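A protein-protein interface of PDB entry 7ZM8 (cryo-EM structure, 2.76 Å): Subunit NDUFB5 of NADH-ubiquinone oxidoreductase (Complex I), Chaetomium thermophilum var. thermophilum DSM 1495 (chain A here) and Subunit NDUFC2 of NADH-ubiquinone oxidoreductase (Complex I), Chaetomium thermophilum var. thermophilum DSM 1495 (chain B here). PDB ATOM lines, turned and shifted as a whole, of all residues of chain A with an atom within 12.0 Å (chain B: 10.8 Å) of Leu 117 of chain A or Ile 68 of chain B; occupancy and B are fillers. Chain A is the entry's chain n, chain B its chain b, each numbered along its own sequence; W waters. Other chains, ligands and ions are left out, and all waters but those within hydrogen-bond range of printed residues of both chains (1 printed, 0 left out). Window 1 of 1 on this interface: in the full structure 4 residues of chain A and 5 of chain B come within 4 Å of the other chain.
OE1 of Gln 110 of chain A lies close to OD1 of Asp 114 of chain A (3.2 Å).
The side-chain amino group of Lys 65 of chain B lies within hydrogen-bond range of the backbone carbonyl oxygen of Leu 61 of chain B (3.1 Å).
NZ of Lys 65 of chain B lies within salt-bridge range of OE2 of Glu 62 of chain B (3.9 Å).
CG of Asp 114 of chain A touches CD of Lys 65 of chain B (3.6 Å).
Leu 117 of chain A touches Lys 65 of chain B (CD2 to O, 3.4 Å).
Ile 68 of chain B touches Leu 117 of chain A (CG2 to CD1, 3.8 Å).
Leu 69 of chain B touches Leu 117 of chain A (CD2 to CD1, 3.8 Å).
CD2 of Leu 118 of chain A touches CG of Arg 64 of chain B, 3.8 Å away.
Lys 65 of chain B touches Leu 118 of chain A (CG to CG, 3.8 Å).
Ile 68 of chain B touches Leu 118 of chain A.
CG of Glu 122 of chain A touches NH2 of Arg 75 of chain B (3.98 Å).
Of chain B, only Lys 65 (3.4 Å), Ile 68 (3.8 Å) and Leu 69 (3.8 Å) come within 4 Å of Leu 117 of chain A.
Printed residues of chain A within 4 Å of Ile 68 of chain B: Leu 117 (3.8 Å) and Leu 118 (3.8 Å).
Of chain B, only Lys 65 comes within 4 Å of Asp 114 of chain A.
No residue of chain B comes within 4 Å of Thr 120 of chain A.
Arg 64 of chain B touches one residue of chain A.
No residue of chain A comes within 4 Å of Gln 66 of chain B.
No residue of chain A comes within 4 Å of Ala 67 of chain B.
No residue of chain A comes within 4 Å of Lys 71 of chain B.
Of the printed residues of chain B, Glu 122 of chain A touches Arg 75 (3.98 Å).
Printed residues of chain A within 4 Å of Arg 75 of chain B: Glu 122.
The nearest residue of chain B that does not touch Leu 117 of chain A is Arg 72 of chain B (4.2 Å).
The nearest printed residue of chain B that does not touch Glu 122 of chain A is Lys 71 of chain B (4.1 Å).
Printed residues of chain B that touch a printed residue of chain A: Arg 64, Lys 65, Ile 68, Leu 69 and Arg 75.
Hydrophobic or aromatic side chains of chain B that line the printed part of chain A: Ile 68 and Leu 69.
Along chain B the printed residues that touch a printed residue of chain A span positions 64 to 75.
Hydrophobic or aromatic side chains of chain A within 4 Å of the printed part of chain B: Leu 117 and Leu 118.
Among the printed residues, 8 pairs touch across the chains.
Among the printed residues, no Asp or Glu carboxylate lies within 4 Å of a Lys or Arg side-chain nitrogen of the other chain.
Water W1 lies within hydrogen-bond range of O of Glu 122 of chain A (2.5 Å) and NH2 of Arg 64 of chain B (3.0 Å).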
ATOM      1  N   LEU A 108     -19.639 -22.900   3.245  1.00  0.00           N
ATOM      2  CA  LEU A 108     -18.455 -22.026   3.427  1.00  0.00           C
ATOM      3  C   LEU A 108     -18.892 -20.752   4.141  1.00  0.00           C
ATOM      4  O   LEU A 108     -18.038 -20.144   4.806  1.00  0.00           O
ATOM      5  CB  LEU A 108     -17.793 -21.791   2.069  1.00  0.00           C
ATOM      6  CG  LEU A 108     -16.880 -22.936   1.638  1.00  0.00           C
ATOM      7  CD1 LEU A 108     -16.911 -23.148   0.138  1.00  0.00           C
ATOM      8  CD2 LEU A 108     -15.462 -22.713   2.131  1.00  0.00           C
ATOM      9  N   GLU A 109     -20.163 -20.370   4.016  1.00  0.00           N
ATOM     10  CA  GLU A 109     -20.693 -19.242   4.815  1.00  0.00           C
ATOM     11  C   GLU A 109     -20.825 -19.677   6.274  1.00  0.00           C
ATOM     12  O   GLU A 109     -20.544 -18.841   7.153  1.00  0.00           O
ATOM     13  CB  GLU A 109     -22.081 -18.867   4.322  1.00  0.00           C
ATOM     14  CG  GLU A 109     -22.086 -17.970   3.101  1.00  0.00           C
ATOM     15  CD  GLU A 109     -21.862 -16.499   3.401  1.00  0.00           C
ATOM     16  OE1 GLU A 109     -21.796 -16.144   4.593  1.00  0.00           O
ATOM     17  OE2 GLU A 109     -21.753 -15.714   2.440  1.00  0.00           O
ATOM     18  N   GLN A 110     -21.242 -20.910   6.539  1.00  0.00           N
ATOM     19  CA  GLN A 110     -21.360 -21.407   7.931  1.00  0.00           C
ATOM     20  C   GLN A 110     -19.975 -21.437   8.571  1.00  0.00           C
ATOM     21  O   GLN A 110     -19.847 -20.990   9.711  1.00  0.00           O
ATOM     22  CB  GLN A 110     -22.020 -22.779   7.988  1.00  0.00           C
ATOM     23  CG  GLN A 110     -22.197 -23.316   9.400  1.00  0.00           C
ATOM     24  CD  GLN A 110     -23.130 -22.470  10.230  1.00  0.00           C
ATOM     25  OE1 GLN A 110     -22.873 -22.190  11.398  1.00  0.00           O
ATOM     26  NE2 GLN A 110     -24.228 -22.047   9.624  1.00  0.00           N
ATOM     27  N   ALA A 111     -18.990 -21.995   7.879  1.00  0.00           N
ATOM     28  CA  ALA A 111     -17.632 -22.148   8.427  1.00  0.00           C
ATOM     29  C   ALA A 111     -17.030 -20.788   8.763  1.00  0.00           C
ATOM     30  O   ALA A 111     -16.237 -20.735   9.704  1.00  0.00           O
ATOM     31  CB  ALA A 111     -16.814 -22.905   7.428  1.00  0.00           C
ATOM     32  N   ALA A 112     -17.330 -19.751   7.990  1.00  0.00           N
ATOM     33  CA  ALA A 112     -16.858 -18.383   8.305  1.00  0.00           C
ATOM     34  C   ALA A 112     -17.412 -17.924   9.659  1.00  0.00           C
ATOM     35  O   ALA A 112     -16.666 -17.287  10.398  1.00  0.00           O
ATOM     36  CB  ALA A 112     -17.338 -17.469   7.217  1.00  0.00           C
ATOM     37  N   HIS A 113     -18.683 -18.207   9.938  1.00  0.00           N
ATOM     38  CA  HIS A 113     -19.329 -17.856  11.220  1.00  0.00           C
ATOM     39  C   HIS A 113     -18.623 -18.650  12.307  1.00  0.00           C
ATOM     40  O   HIS A 113     -18.361 -18.077  13.377  1.00  0.00           O
ATOM     41  CB  HIS A 113     -20.808 -18.243  11.121  1.00  0.00           C
ATOM     42  CG  HIS A 113     -21.618 -18.050  12.353  1.00  0.00           C
ATOM     43  ND1 HIS A 113     -22.622 -17.113  12.419  1.00  0.00           N
ATOM     44  CD2 HIS A 113     -21.618 -18.695  13.539  1.00  0.00           C
ATOM     45  CE1 HIS A 113     -23.198 -17.172  13.600  1.00  0.00           C
ATOM     46  NE2 HIS A 113     -22.597 -18.134  14.308  1.00  0.00           N
ATOM     47  N   ASP A 114     -18.322 -19.918  12.033  1.00  0.00           N
ATOM     48  CA  ASP A 114     -17.674 -20.810  13.030  1.00  0.00           C
ATOM     49  C   ASP A 114     -16.256 -20.319  13.310  1.00  0.00           C
ATOM     50  O   ASP A 114     -15.882 -20.309  14.482  1.00  0.00           O
ATOM     51  CB  ASP A 114     -17.803 -22.273  12.622  1.00  0.00           C
ATOM     52  CG  ASP A 114     -19.239 -22.754  12.638  1.00  0.00           C
ATOM     53  OD1 ASP A 114     -20.112 -21.953  13.015  1.00  0.00           O
ATOM     54  OD2 ASP A 114     -19.470 -23.925  12.281  1.00  0.00           O
ATOM     55  N   LYS A 115     -15.493 -19.999  12.267  1.00  0.00           N
ATOM     56  CA  LYS A 115     -14.092 -19.531  12.414  1.00  0.00           C
ATOM     57  C   LYS A 115     -14.092 -18.276  13.268  1.00  0.00           C
ATOM     58  O   LYS A 115     -13.173 -18.126  14.072  1.00  0.00           O
ATOM     59  CB  LYS A 115     -13.474 -19.230  11.047  1.00  0.00           C
ATOM     60  CG  LYS A 115     -12.196 -18.403  11.050  1.00  0.00           C
ATOM     61  CD  LYS A 115     -11.681 -18.108   9.662  1.00  0.00           C
ATOM     62  CE  LYS A 115     -10.647 -17.003   9.622  1.00  0.00           C
ATOM     63  NZ  LYS A 115     -10.216 -16.708   8.236  1.00  0.00           N
ATOM     64  N   HIS A 116     -15.135 -17.459  13.150  1.00  0.00           N
ATOM     65  CA  HIS A 116     -15.213 -16.193  13.909  1.00  0.00           C
ATOM     66  C   HIS A 116     -15.574 -16.545  15.352  1.00  0.00           C
ATOM     67  O   HIS A 116     -15.016 -15.944  16.241  1.00  0.00           O
ATOM     68  CB  HIS A 116     -16.281 -15.296  13.277  1.00  0.00           C
ATOM     69  CG  HIS A 116     -15.783 -14.353  12.238  1.00  0.00           C
ATOM     70  ND1 HIS A 116     -16.621 -13.465  11.599  1.00  0.00           N
ATOM     71  CD2 HIS A 116     -14.553 -14.142  11.729  1.00  0.00           C
ATOM     72  CE1 HIS A 116     -15.930 -12.749  10.740  1.00  0.00           C
ATOM     73  NE2 HIS A 116     -14.663 -13.144  10.803  1.00  0.00           N
ATOM     74  N   LEU A 117     -16.444 -17.534  15.558  1.00  0.00           N
ATOM     75  CA  LEU A 117     -16.870 -17.906  16.936  1.00  0.00           C
ATOM     76  C   LEU A 117     -15.702 -18.496  17.726  1.00  0.00           C
ATOM     77  O   LEU A 117     -15.498 -18.085  18.864  1.00  0.00           O
ATOM     78  CB  LEU A 117     -18.023 -18.906  16.820  1.00  0.00           C
ATOM     79  CG  LEU A 117     -18.649 -19.370  18.131  1.00  0.00           C
ATOM     80  CD1 LEU A 117     -19.516 -18.274  18.728  1.00  0.00           C
ATOM     81  CD2 LEU A 117     -19.461 -20.632  17.909  1.00  0.00           C
ATOM     82  N   LEU A 118     -14.940 -19.400  17.116  1.00  0.00           N
ATOM     83  CA  LEU A 118     -13.823 -20.073  17.821  1.00  0.00           C
ATOM     84  C   LEU A 118     -12.648 -19.113  18.020  1.00  0.00           C
ATOM     85  O   LEU A 118     -11.991 -19.220  19.061  1.00  0.00           O
ATOM     86  CB  LEU A 118     -13.403 -21.296  17.005  1.00  0.00           C
ATOM     87  CG  LEU A 118     -14.367 -22.479  17.009  1.00  0.00           C
ATOM     88  CD1 LEU A 118     -14.106 -23.379  15.811  1.00  0.00           C
ATOM     89  CD2 LEU A 118     -14.250 -23.270  18.299  1.00  0.00           C
ATOM     90  N   LEU A 119     -12.404 -18.206  17.076  1.00  0.00           N
ATOM     91  CA  LEU A 119     -11.203 -17.328  17.146  1.00  0.00           C
ATOM     92  C   LEU A 119     -11.458 -16.064  17.974  1.00  0.00           C
ATOM     93  O   LEU A 119     -10.479 -15.353  18.243  1.00  0.00           O
ATOM     94  CB  LEU A 119     -10.783 -16.970  15.717  1.00  0.00           C
ATOM     95  CG  LEU A 119      -9.345 -17.293  15.325  1.00  0.00           C
ATOM     96  CD1 LEU A 119      -8.979 -18.711  15.722  1.00  0.00           C
ATOM     97  CD2 LEU A 119      -9.153 -17.096  13.832  1.00  0.00           C
ATOM     98  N   THR A 120     -12.708 -15.774  18.331  1.00  0.00           N
ATOM     99  CA  THR A 120     -13.008 -14.508  19.052  1.00  0.00           C
ATOM    100  C   THR A 120     -13.673 -14.860  20.373  1.00  0.00           C
ATOM    101  O   THR A 120     -14.601 -14.137  20.769  1.00  0.00           O
ATOM    102  CB  THR A 120     -13.911 -13.555  18.255  1.00  0.00           C
ATOM    103  OG1 THR A 120     -15.195 -14.152  18.084  1.00  0.00           O
ATOM    104  CG2 THR A 120     -13.337 -13.146  16.918  1.00  0.00           C
ATOM    105  N   ALA A 121     -13.176 -15.893  21.050  1.00  0.00           N
ATOM    106  CA  ALA A 121     -13.857 -16.362  22.261  1.00  0.00           C
ATOM    107  C   ALA A 121     -13.262 -15.722  23.509  1.00  0.00           C
ATOM    108  O   ALA A 121     -12.112 -15.298  23.458  1.00  0.00           O
ATOM    109  CB  ALA A 121     -13.853 -17.869  22.277  1.00  0.00           C
ATOM    110  N   GLU A 122     -14.059 -15.624  24.569  1.00  0.00           N
ATOM    111  CA  GLU A 122     -13.593 -14.961  25.805  1.00  0.00           C
ATOM    112  C   GLU A 122     -12.423 -15.749  26.398  1.00  0.00           C
ATOM    113  O   GLU A 122     -12.534 -16.962  26.525  1.00  0.00           O
ATOM    114  CB  GLU A 122     -14.762 -14.835  26.780  1.00  0.00           C
ATOM    115  CG  GLU A 122     -14.424 -14.083  28.054  1.00  0.00           C
ATOM    116  CD  GLU A 122     -14.231 -12.585  27.892  1.00  0.00           C
ATOM    117  OE1 GLU A 122     -14.679 -12.037  26.865  1.00  0.00           O
ATOM    118  OE2 GLU A 122     -13.633 -11.969  28.795  1.00  0.00           O
ATOM    119  N   ARG A 123     -11.348 -15.059  26.748  1.00  0.00           N
ATOM    120  CA  ARG A 123     -10.191 -15.709  27.398  1.00  0.00           C
ATOM    121  C   ARG A 123     -10.572 -15.845  28.862  1.00  0.00           C
ATOM    122  O   ARG A 123     -11.252 -14.946  29.371  1.00  0.00           O
ATOM    123  CB  ARG A 123      -8.973 -14.787  27.274  1.00  0.00           C
ATOM    124  CG  ARG A 123      -7.652 -15.353  27.761  1.00  0.00           C
ATOM    125  CD  ARG A 123      -6.666 -14.208  27.864  1.00  0.00           C
ATOM    126  NE  ARG A 123      -5.288 -14.660  27.942  1.00  0.00           N
ATOM    127  CZ  ARG A 123      -4.418 -14.571  26.947  1.00  0.00           C
ATOM    128  NH1 ARG A 123      -4.778 -14.020  25.802  1.00  0.00           N
ATOM    129  NH2 ARG A 123      -3.188 -15.016  27.107  1.00  0.00           N
ATOM    130  N   SER A 124     -10.147 -16.928  29.498  1.00  0.00           N
ATOM    131  CA  SER A 124     -10.424 -17.125  30.934  1.00  0.00           C
ATOM    132  C   SER A 124      -9.768 -16.015  31.734  1.00  0.00           C
ATOM    133  O   SER A 124      -8.606 -15.689  31.460  1.00  0.00           O
ATOM    134  CB  SER A 124      -9.938 -18.449  31.378  1.00  0.00           C
ATOM    135  OG  SER A 124      -8.534 -18.541  31.222  1.00  0.00           O
ATOM    136  N   MET B  60     -15.773 -33.053  19.170  1.00  0.00           N
ATOM    137  CA  MET B  60     -15.356 -32.145  20.229  1.00  0.00           C
ATOM    138  C   MET B  60     -15.301 -30.701  19.749  1.00  0.00           C
ATOM    139  O   MET B  60     -15.568 -29.780  20.526  1.00  0.00           O
ATOM    140  CB  MET B  60     -14.015 -32.595  20.801  1.00  0.00           C
ATOM    141  CG  MET B  60     -13.755 -32.035  22.183  1.00  0.00           C
ATOM    142  SD  MET B  60     -12.016 -31.873  22.573  1.00  0.00           S
ATOM    143  CE  MET B  60     -11.646 -33.596  22.866  1.00  0.00           C
ATOM    144  N   LEU B  61     -14.954 -30.473  18.484  1.00  0.00           N
ATOM    145  CA  LEU B  61     -15.038 -29.115  17.965  1.00  0.00           C
ATOM    146  C   LEU B  61     -16.483 -28.669  17.816  1.00  0.00           C
ATOM    147  O   LEU B  61     -16.775 -27.477  17.949  1.00  0.00           O
ATOM    148  CB  LEU B  61     -14.305 -29.003  16.629  1.00  0.00           C
ATOM    149  CG  LEU B  61     -12.788 -28.868  16.725  1.00  0.00           C
ATOM    150  CD1 LEU B  61     -12.156 -28.960  15.357  1.00  0.00           C
ATOM    151  CD2 LEU B  61     -12.411 -27.572  17.410  1.00  0.00           C
ATOM    152  N   GLU B  62     -17.394 -29.599  17.532  1.00  0.00           N
ATOM    153  CA  GLU B  62     -18.811 -29.260  17.511  1.00  0.00           C
ATOM    154  C   GLU B  62     -19.304 -28.867  18.894  1.00  0.00           C
ATOM    155  O   GLU B  62     -20.042 -27.886  19.043  1.00  0.00           O
ATOM    156  CB  GLU B  62     -19.625 -30.434  16.973  1.00  0.00           C
ATOM    157  CG  GLU B  62     -19.753 -30.455  15.464  1.00  0.00           C
ATOM    158  CD  GLU B  62     -20.553 -29.284  14.929  1.00  0.00           C
ATOM    159  OE1 GLU B  62     -21.585 -28.942  15.541  1.00  0.00           O
ATOM    160  OE2 GLU B  62     -20.147 -28.706  13.899  1.00  0.00           O
ATOM    161  N   GLU B  63     -18.952 -29.643  19.917  1.00  0.00           N
ATOM    162  CA  GLU B  63     -19.326 -29.330  21.322  1.00  0.00           C
ATOM    163  C   GLU B  63     -18.843 -27.937  21.705  1.00  0.00           C
ATOM    164  O   GLU B  63     -19.617 -27.222  22.332  1.00  0.00           O
ATOM    165  CB  GLU B  63     -18.719 -30.355  22.274  1.00  0.00           C
ATOM    166  CG  GLU B  63     -19.422 -31.699  22.253  1.00  0.00           C
ATOM    167  CD  GLU B  63     -20.846 -31.696  22.781  1.00  0.00           C
ATOM    168  OE1 GLU B  63     -21.114 -30.977  23.766  1.00  0.00           O
ATOM    169  OE2 GLU B  63     -21.687 -32.412  22.203  1.00  0.00           O
ATOM    170  N   ARG B  64     -17.584 -27.609  21.416  1.00  0.00           N
ATOM    171  CA  ARG B  64     -16.989 -26.312  21.812  1.00  0.00           C
ATOM    172  C   ARG B  64     -17.786 -25.167  21.191  1.00  0.00           C
ATOM    173  O   ARG B  64     -18.010 -24.175  21.873  1.00  0.00           O
ATOM    174  CB  ARG B  64     -15.533 -26.260  21.350  1.00  0.00           C
ATOM    175  CG  ARG B  64     -14.795 -24.974  21.682  1.00  0.00           C
ATOM    176  CD  ARG B  64     -14.825 -24.605  23.149  1.00  0.00           C
ATOM    177  NE  ARG B  64     -13.902 -23.504  23.353  1.00  0.00           N
ATOM    178  CZ  ARG B  64     -14.038 -22.550  24.258  1.00  0.00           C
ATOM    179  NH1 ARG B  64     -15.086 -22.535  25.061  1.00  0.00           N
ATOM    180  NH2 ARG B  64     -13.129 -21.600  24.341  1.00  0.00           N
ATOM    181  N   LYS B  65     -18.182 -25.309  19.935  1.00  0.00           N
ATOM    182  CA  LYS B  65     -18.902 -24.209  19.281  1.00  0.00           C
ATOM    183  C   LYS B  65     -20.256 -24.074  19.957  1.00  0.00           C
ATOM    184  O   LYS B  65     -20.771 -22.969  20.023  1.00  0.00           O
ATOM    185  CB  LYS B  65     -19.018 -24.508  17.788  1.00  0.00           C
ATOM    186  CG  LYS B  65     -17.720 -24.354  17.012  1.00  0.00           C
ATOM    187  CD  LYS B  65     -17.913 -24.498  15.534  1.00  0.00           C
ATOM    188  CE  LYS B  65     -18.232 -25.914  15.112  1.00  0.00           C
ATOM    189  NZ  LYS B  65     -17.002 -26.725  14.986  1.00  0.00           N
ATOM    190  N   GLN B  66     -20.780 -25.179  20.469  1.00  0.00           N
ATOM    191  CA  GLN B  66     -22.022 -25.106  21.227  1.00  0.00           C
ATOM    192  C   GLN B  66     -21.797 -24.470  22.593  1.00  0.00           C
ATOM    193  O   GLN B  66     -22.647 -23.721  23.078  1.00  0.00           O
ATOM    194  CB  GLN B  66     -22.627 -26.494  21.368  1.00  0.00           C
ATOM    195  CG  GLN B  66     -23.517 -26.877  20.209  1.00  0.00           C
ATOM    196  CD  GLN B  66     -24.509 -25.788  19.861  1.00  0.00           C
ATOM    197  OE1 GLN B  66     -24.377 -25.117  18.839  1.00  0.00           O
ATOM    198  NE2 GLN B  66     -25.507 -25.603  20.716  1.00  0.00           N
ATOM    199  N   ALA B  67     -20.639 -24.705  23.207  1.00  0.00           N
ATOM    200  CA  ALA B  67     -20.314 -24.076  24.507  1.00  0.00           C
ATOM    201  C   ALA B  67     -20.146 -22.556  24.384  1.00  0.00           C
ATOM    202  O   ALA B  67     -20.683 -21.846  25.237  1.00  0.00           O
ATOM    203  CB  ALA B  67     -19.074 -24.700  25.069  1.00  0.00           C
ATOM    204  N   ILE B  68     -19.415 -22.077  23.376  1.00  0.00           N
ATOM    205  CA  ILE B  68     -19.150 -20.622  23.214  1.00  0.00           C
ATOM    206  C   ILE B  68     -20.502 -19.953  22.992  1.00  0.00           C
ATOM    207  O   ILE B  68     -20.650 -18.791  23.369  1.00  0.00           O
ATOM    208  CB  ILE B  68     -18.128 -20.352  22.087  1.00  0.00           C
ATOM    209  CG1 ILE B  68     -16.883 -21.229  22.210  1.00  0.00           C
ATOM    210  CG2 ILE B  68     -17.758 -18.881  22.008  1.00  0.00           C
ATOM    211  CD1 ILE B  68     -16.052 -21.285  20.950  1.00  0.00           C
ATOM    212  N   LEU B  69     -21.472 -20.691  22.465  1.00  0.00           N
ATOM    213  CA  LEU B  69     -22.813 -20.121  22.169  1.00  0.00           C
ATOM    214  C   LEU B  69     -23.689 -20.130  23.422  1.00  0.00           C
ATOM    215  O   LEU B  69     -24.531 -19.242  23.518  1.00  0.00           O
ATOM    216  CB  LEU B  69     -23.440 -20.869  20.987  1.00  0.00           C
ATOM    217  CG  LEU B  69     -22.889 -20.492  19.617  1.00  0.00           C
ATOM    218  CD1 LEU B  69     -23.471 -21.386  18.538  1.00  0.00           C
ATOM    219  CD2 LEU B  69     -23.172 -19.033  19.310  1.00  0.00           C
ATOM    220  N   GLU B  70     -23.538 -21.110  24.315  1.00  0.00           N
ATOM    221  CA  GLU B  70     -24.228 -21.025  25.600  1.00  0.00           C
ATOM    222  C   GLU B  70     -23.628 -19.940  26.481  1.00  0.00           C
ATOM    223  O   GLU B  70     -24.357 -19.216  27.164  1.00  0.00           O
ATOM    224  CB  GLU B  70     -24.205 -22.370  26.327  1.00  0.00           C
ATOM    225  CG  GLU B  70     -24.456 -23.591  25.460  1.00  0.00           C
ATOM    226  CD  GLU B  70     -25.833 -23.613  24.802  1.00  0.00           C
ATOM    227  OE1 GLU B  70     -26.649 -22.695  25.030  1.00  0.00           O
ATOM    228  OE2 GLU B  70     -26.101 -24.566  24.040  1.00  0.00           O
ATOM    229  N   LYS B  71     -22.308 -19.800  26.471  1.00  0.00           N
ATOM    230  CA  LYS B  71     -21.680 -18.732  27.288  1.00  0.00           C
ATOM    231  C   LYS B  71     -22.162 -17.365  26.805  1.00  0.00           C
ATOM    232  O   LYS B  71     -22.580 -16.568  27.653  1.00  0.00           O
ATOM    233  CB  LYS B  71     -20.155 -18.842  27.238  1.00  0.00           C
ATOM    234  CG  LYS B  71     -19.405 -17.885  28.154  1.00  0.00           C
ATOM    235  CD  LYS B  71     -17.931 -18.199  28.269  1.00  0.00           C
ATOM    236  CE  LYS B  71     -17.183 -17.190  29.112  1.00  0.00           C
ATOM    237  NZ  LYS B  71     -17.862 -16.958  30.409  1.00  0.00           N
ATOM    238  N   ARG B  72     -22.100 -17.105  25.501  1.00  0.00           N
ATOM    239  CA  ARG B  72     -22.483 -15.788  24.940  1.00  0.00           C
ATOM    240  C   ARG B  72     -23.962 -15.537  25.215  1.00  0.00           C
ATOM    241  O   ARG B  72     -24.352 -14.362  25.254  1.00  0.00           O
ATOM    242  CB  ARG B  72     -22.214 -15.761  23.436  1.00  0.00           C
ATOM    243  CG  ARG B  72     -20.741 -15.704  23.065  1.00  0.00           C
ATOM    244  CD  ARG B  72     -20.589 -15.425  21.585  1.00  0.00           C
ATOM    245  NE  ARG B  72     -21.425 -14.289  21.235  1.00  0.00           N
ATOM    246  CZ  ARG B  72     -21.054 -13.020  21.350  1.00  0.00           C
ATOM    247  NH1 ARG B  72     -19.846 -12.721  21.794  1.00  0.00           N
ATOM    248  NH2 ARG B  72     -21.887 -12.056  21.008  1.00  0.00           N
ATOM    249  N   ALA B  73     -24.746 -16.597  25.397  1.00  0.00           N
ATOM    250  CA  ALA B  73     -26.203 -16.463  25.589  1.00  0.00           C
ATOM    251  C   ALA B  73     -26.509 -16.309  27.074  1.00  0.00           C
ATOM    252  O   ALA B  73     -27.292 -15.418  27.406  1.00  0.00           O
ATOM    253  CB  ALA B  73     -26.890 -17.672  25.016  1.00  0.00           C
ATOM    254  N   ARG B  74     -25.927 -17.147  27.932  1.00  0.00           N
ATOM    255  CA  ARG B  74     -26.114 -16.952  29.366  1.00  0.00           C
ATOM    256  C   ARG B  74     -25.677 -15.560  29.794  1.00  0.00           C
ATOM    257  O   ARG B  74     -26.334 -14.926  30.625  1.00  0.00           O
ATOM    258  CB  ARG B  74     -25.342 -18.016  30.146  1.00  0.00           C
ATOM    259  CG  ARG B  74     -26.069 -19.339  30.277  1.00  0.00           C
ATOM    260  CD  ARG B  74     -25.269 -20.324  31.107  1.00  0.00           C
ATOM    261  NE  ARG B  74     -24.075 -20.787  30.406  1.00  0.00           N
ATOM    262  CZ  ARG B  74     -22.834 -20.452  30.743  1.00  0.00           C
ATOM    263  NH1 ARG B  74     -22.623 -19.647  31.774  1.00  0.00           N
ATOM    264  NH2 ARG B  74     -21.807 -20.922  30.052  1.00  0.00           N
ATOM    265  N   ARG B  75     -24.560 -15.077  29.250  1.00  0.00           N
ATOM    266  CA  ARG B  75     -24.120 -13.721  29.546  1.00  0.00           C
ATOM    267  C   ARG B  75     -25.107 -12.697  29.010  1.00  0.00           C
ATOM    268  O   ARG B  75     -25.406 -11.703  29.680  1.00  0.00           O
ATOM    269  CB  ARG B  75     -22.728 -13.483  28.963  1.00  0.00           C
ATOM    270  CG  ARG B  75     -22.161 -12.110  29.251  1.00  0.00           C
ATOM    271  CD  ARG B  75     -20.986 -11.801  28.338  1.00  0.00           C
ATOM    272  NE  ARG B  75     -19.901 -12.767  28.493  1.00  0.00           N
ATOM    273  CZ  ARG B  75     -19.040 -12.774  29.507  1.00  0.00           C
ATOM    274  NH1 ARG B  75     -19.130 -11.862  30.465  1.00  0.00           N
ATOM    275  NH2 ARG B  75     -18.086 -13.692  29.562  1.00  0.00           N
ATOM    276  N   ALA B  76     -25.625 -12.919  27.802  1.00  0.00           N
ATOM    277  CA  ALA B  76     -26.606 -11.997  27.242  1.00  0.00           C
ATOM    278  C   ALA B  76     -27.883 -11.986  28.068  1.00  0.00           C
ATOM    279  O   ALA B  76     -28.492 -10.930  28.270  1.00  0.00           O
ATOM    280  CB  ALA B  76     -26.910 -12.366  25.792  1.00  0.00           C
HETATM  281  O   HOH W   1     -13.492 -19.236  26.068  1.00  0.00           O
